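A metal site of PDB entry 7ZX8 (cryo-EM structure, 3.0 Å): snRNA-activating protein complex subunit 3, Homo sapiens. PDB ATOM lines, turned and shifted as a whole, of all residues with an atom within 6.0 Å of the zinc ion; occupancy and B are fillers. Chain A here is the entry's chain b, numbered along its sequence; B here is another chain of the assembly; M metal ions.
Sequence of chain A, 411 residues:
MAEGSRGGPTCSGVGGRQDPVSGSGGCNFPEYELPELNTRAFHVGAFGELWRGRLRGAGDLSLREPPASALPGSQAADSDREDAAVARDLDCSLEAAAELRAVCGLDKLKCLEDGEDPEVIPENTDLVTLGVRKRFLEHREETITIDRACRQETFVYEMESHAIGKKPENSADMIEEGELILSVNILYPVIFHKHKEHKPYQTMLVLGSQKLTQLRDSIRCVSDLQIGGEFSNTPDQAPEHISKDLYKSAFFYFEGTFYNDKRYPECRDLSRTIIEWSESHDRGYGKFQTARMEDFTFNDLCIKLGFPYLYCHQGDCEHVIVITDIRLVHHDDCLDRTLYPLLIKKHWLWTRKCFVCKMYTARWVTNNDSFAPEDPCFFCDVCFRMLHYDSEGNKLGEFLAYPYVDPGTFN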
ATOM      1  N   CYS A 354     -20.438  -7.949   5.734  1.00  0.00           N
ATOM      2  CA  CYS A 354     -21.491  -7.170   5.096  1.00  0.00           C
ATOM      3  C   CYS A 354     -22.144  -7.988   3.998  1.00  0.00           C
ATOM      4  O   CYS A 354     -21.552  -8.902   3.420  1.00  0.00           O
ATOM      5  CB  CYS A 354     -20.919  -5.879   4.512  1.00  0.00           C
ATOM      6  SG  CYS A 354     -21.989  -5.018   3.358  1.00  0.00           S
ATOM      7  N   PHE A 355     -23.408  -7.662   3.697  1.00  0.00           N
ATOM      8  CA  PHE A 355     -24.153  -8.423   2.715  1.00  0.00           C
ATOM      9  C   PHE A 355     -24.112  -7.808   1.331  1.00  0.00           C
ATOM     10  O   PHE A 355     -24.290  -8.514   0.347  1.00  0.00           O
ATOM     11  CB  PHE A 355     -25.593  -8.616   3.167  1.00  0.00           C
ATOM     12  CG  PHE A 355     -25.788  -9.831   4.006  1.00  0.00           C
ATOM     13  CD1 PHE A 355     -24.723 -10.380   4.702  1.00  0.00           C
ATOM     14  CD2 PHE A 355     -27.030 -10.427   4.099  1.00  0.00           C
ATOM     15  CE1 PHE A 355     -24.898 -11.497   5.481  1.00  0.00           C
ATOM     16  CE2 PHE A 355     -27.206 -11.553   4.873  1.00  0.00           C
ATOM     17  CZ  PHE A 355     -26.136 -12.088   5.562  1.00  0.00           C
ATOM     18  N   VAL A 356     -23.894  -6.502   1.239  1.00  0.00           N
ATOM     19  CA  VAL A 356     -23.731  -5.835  -0.045  1.00  0.00           C
ATOM     20  C   VAL A 356     -22.331  -6.066  -0.592  1.00  0.00           C
ATOM     21  O   VAL A 356     -22.174  -6.669  -1.659  1.00  0.00           O
ATOM     22  CB  VAL A 356     -24.027  -4.327   0.076  1.00  0.00           C
ATOM     23  CG1 VAL A 356     -24.168  -3.730  -1.303  1.00  0.00           C
ATOM     24  CG2 VAL A 356     -25.265  -4.106   0.891  1.00  0.00           C
ATOM     25  N   CYS A 357     -21.316  -5.606   0.117  1.00  0.00           N
ATOM     26  CA  CYS A 357     -19.930  -5.922  -0.199  1.00  0.00           C
ATOM     27  C   CYS A 357     -19.466  -6.987   0.775  1.00  0.00           C
ATOM     28  O   CYS A 357     -20.009  -7.105   1.879  1.00  0.00           O
ATOM     29  CB  CYS A 357     -19.044  -4.683  -0.096  1.00  0.00           C
ATOM     30  SG  CYS A 357     -19.150  -3.894   1.512  1.00  0.00           S
ATOM     31  N   LYS A 358     -18.476  -7.762   0.369  1.00  0.00           N
ATOM     32  CA  LYS A 358     -17.939  -8.826   1.210  1.00  0.00           C
ATOM     33  C   LYS A 358     -16.544  -8.504   1.716  1.00  0.00           C
ATOM     34  O   LYS A 358     -15.790  -9.397   2.102  1.00  0.00           O
ATOM     35  CB  LYS A 358     -17.940 -10.146   0.464  1.00  0.00           C
ATOM     36  CG  LYS A 358     -19.293 -10.551  -0.070  1.00  0.00           C
ATOM     37  CD  LYS A 358     -20.332 -10.426   1.013  1.00  0.00           C
ATOM     38  CE  LYS A 358     -21.519 -11.334   0.727  1.00  0.00           C
ATOM     39  NZ  LYS A 358     -21.122 -12.764   0.793  1.00  0.00           N
ATOM     40  N   TYR A 360     -15.816  -6.267   4.276  1.00  0.00           N
ATOM     41  CA  TYR A 360     -15.800  -5.713   5.619  1.00  0.00           C
ATOM     42  C   TYR A 360     -16.778  -6.477   6.482  1.00  0.00           C
ATOM     43  O   TYR A 360     -17.559  -7.309   5.990  1.00  0.00           O
ATOM     44  CB  TYR A 360     -16.123  -4.214   5.615  1.00  0.00           C
ATOM     45  CG  TYR A 360     -15.245  -3.413   4.693  1.00  0.00           C
ATOM     46  CD1 TYR A 360     -14.063  -2.851   5.158  1.00  0.00           C
ATOM     47  CD2 TYR A 360     -15.578  -3.223   3.363  1.00  0.00           C
ATOM     48  CE1 TYR A 360     -13.254  -2.127   4.317  1.00  0.00           C
ATOM     49  CE2 TYR A 360     -14.765  -2.512   2.525  1.00  0.00           C
ATOM     50  CZ  TYR A 360     -13.610  -1.963   3.001  1.00  0.00           C
ATOM     51  OH  TYR A 360     -12.796  -1.244   2.167  1.00  0.00           O
ATOM     52  N   PHE A 379     -25.020  -5.212   7.351  1.00  0.00           N
ATOM     53  CA  PHE A 379     -24.354  -4.236   6.512  1.00  0.00           C
ATOM     54  C   PHE A 379     -23.118  -3.718   7.214  1.00  0.00           C
ATOM     55  O   PHE A 379     -23.166  -3.396   8.410  1.00  0.00           O
ATOM     56  CB  PHE A 379     -25.269  -3.062   6.185  1.00  0.00           C
ATOM     57  CG  PHE A 379     -26.499  -3.439   5.431  1.00  0.00           C
ATOM     58  CD1 PHE A 379     -26.544  -3.307   4.056  1.00  0.00           C
ATOM     59  CD2 PHE A 379     -27.612  -3.908   6.084  1.00  0.00           C
ATOM     60  CE1 PHE A 379     -27.667  -3.639   3.355  1.00  0.00           C
ATOM     61  CE2 PHE A 379     -28.744  -4.241   5.387  1.00  0.00           C
ATOM     62  CZ  PHE A 379     -28.771  -4.117   4.022  1.00  0.00           C
ATOM     63  N   CYS A 380     -22.015  -3.631   6.487  1.00  0.00           N
ATOM     64  CA  CYS A 380     -20.893  -2.840   6.949  1.00  0.00           C
ATOM     65  C   CYS A 380     -21.297  -1.375   7.035  1.00  0.00           C
ATOM     66  O   CYS A 380     -22.294  -0.960   6.439  1.00  0.00           O
ATOM     67  CB  CYS A 380     -19.705  -2.987   6.010  1.00  0.00           C
ATOM     68  SG  CYS A 380     -20.018  -2.320   4.382  1.00  0.00           S
ATOM     69  N   ASP A 381     -20.517  -0.601   7.766  1.00  0.00           N
ATOM     70  CA  ASP A 381     -20.897   0.785   7.992  1.00  0.00           C
ATOM     71  C   ASP A 381     -20.915   1.572   6.691  1.00  0.00           C
ATOM     72  O   ASP A 381     -21.787   2.420   6.469  1.00  0.00           O
ATOM     73  CB  ASP A 381     -19.951   1.427   9.005  1.00  0.00           C
ATOM     74  CG  ASP A 381     -20.552   2.644   9.662  1.00  0.00           C
ATOM     75  OD1 ASP A 381     -21.452   2.471  10.509  1.00  0.00           O
ATOM     76  OD2 ASP A 381     -20.144   3.770   9.333  1.00  0.00           O
ATOM     77  N   VAL A 382     -19.970   1.280   5.801  1.00  0.00           N
ATOM     78  CA  VAL A 382     -19.875   2.006   4.534  1.00  0.00           C
ATOM     79  C   VAL A 382     -21.190   1.932   3.774  1.00  0.00           C
ATOM     80  O   VAL A 382     -21.839   2.945   3.517  1.00  0.00           O
ATOM     81  CB  VAL A 382     -18.712   1.469   3.691  1.00  0.00           C
ATOM     82  CG1 VAL A 382     -18.757   2.058   2.295  1.00  0.00           C
ATOM     83  CG2 VAL A 382     -17.390   1.781   4.366  1.00  0.00           C
ATOM     84  N   CYS A 383     -21.601   0.717   3.411  1.00  0.00           N
ATOM     85  CA  CYS A 383     -22.796   0.580   2.581  1.00  0.00           C
ATOM     86  C   CYS A 383     -24.063   0.870   3.363  1.00  0.00           C
ATOM     87  O   CYS A 383     -25.027   1.415   2.815  1.00  0.00           O
ATOM     88  CB  CYS A 383     -22.841  -0.810   1.959  1.00  0.00           C
ATOM     89  SG  CYS A 383     -21.263  -1.315   1.248  1.00  0.00           S
ATOM     90  N   PHE A 384     -24.084   0.510   4.650  1.00  0.00           N
ATOM     91  CA  PHE A 384     -25.217   0.897   5.485  1.00  0.00           C
ATOM     92  C   PHE A 384     -25.478   2.391   5.407  1.00  0.00           C
ATOM     93  O   PHE A 384     -26.627   2.835   5.407  1.00  0.00           O
ATOM     94  CB  PHE A 384     -24.972   0.489   6.928  1.00  0.00           C
ATOM     95  CG  PHE A 384     -25.989   1.026   7.876  1.00  0.00           C
ATOM     96  CD1 PHE A 384     -27.245   0.472   7.937  1.00  0.00           C
ATOM     97  CD2 PHE A 384     -25.687   2.090   8.687  1.00  0.00           C
ATOM     98  CE1 PHE A 384     -28.187   0.960   8.802  1.00  0.00           C
ATOM     99  CE2 PHE A 384     -26.623   2.582   9.563  1.00  0.00           C
ATOM    100  CZ  PHE A 384     -27.880   2.019   9.620  1.00  0.00           C
ATOM    101  N   GLN B 338     -20.300  -1.727  -5.797  1.00  0.00           N
ATOM    102  CA  GLN B 338     -19.228  -2.032  -4.851  1.00  0.00           C
ATOM    103  C   GLN B 338     -18.248  -3.044  -5.432  1.00  0.00           C
ATOM    104  O   GLN B 338     -17.035  -2.840  -5.359  1.00  0.00           O
ATOM    105  CB  GLN B 338     -19.825  -2.566  -3.551  1.00  0.00           C
ATOM    106  CG  GLN B 338     -20.729  -1.585  -2.850  1.00  0.00           C
ATOM    107  CD  GLN B 338     -19.979  -0.427  -2.249  1.00  0.00           C
ATOM    108  OE1 GLN B 338     -19.787   0.600  -2.905  1.00  0.00           O
ATOM    109  NE2 GLN B 338     -19.570  -0.567  -0.995  1.00  0.00           N
HETATM  110 ZN    ZN M   1     -20.989  -3.090   2.668  1.00  0.00          ZN
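N of Val 356 lies close to SG of Cys 354 (3.2 Å).
N of Cys 354 lies within hydrogen-bond range of O of Tyr 360 (3.0 Å).
The side-chain amide nitrogen (NE2) of Gln 338 of chain B lies close to the side-chain sulfur (SG) of Cys 383 (2.9 Å).
Of the 13 residues printed, 4 come within 4 Å of the zinc ion.
The nearest printed residue that does not touch the zinc ion is Val 356 (4.2 Å).
SG of Cys 380 binds the zinc ion, 2.1 Å away.
The zinc ion is bound by SG of Cys 354 (2.3 Å).
The zinc ion is bound by the side-chain sulfur (SG) of Cys 383, at 2.3 Å.
SG of Cys 357 binds the zinc ion (2.3 Å).
The zinc ion has four donor atoms within binding distance.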
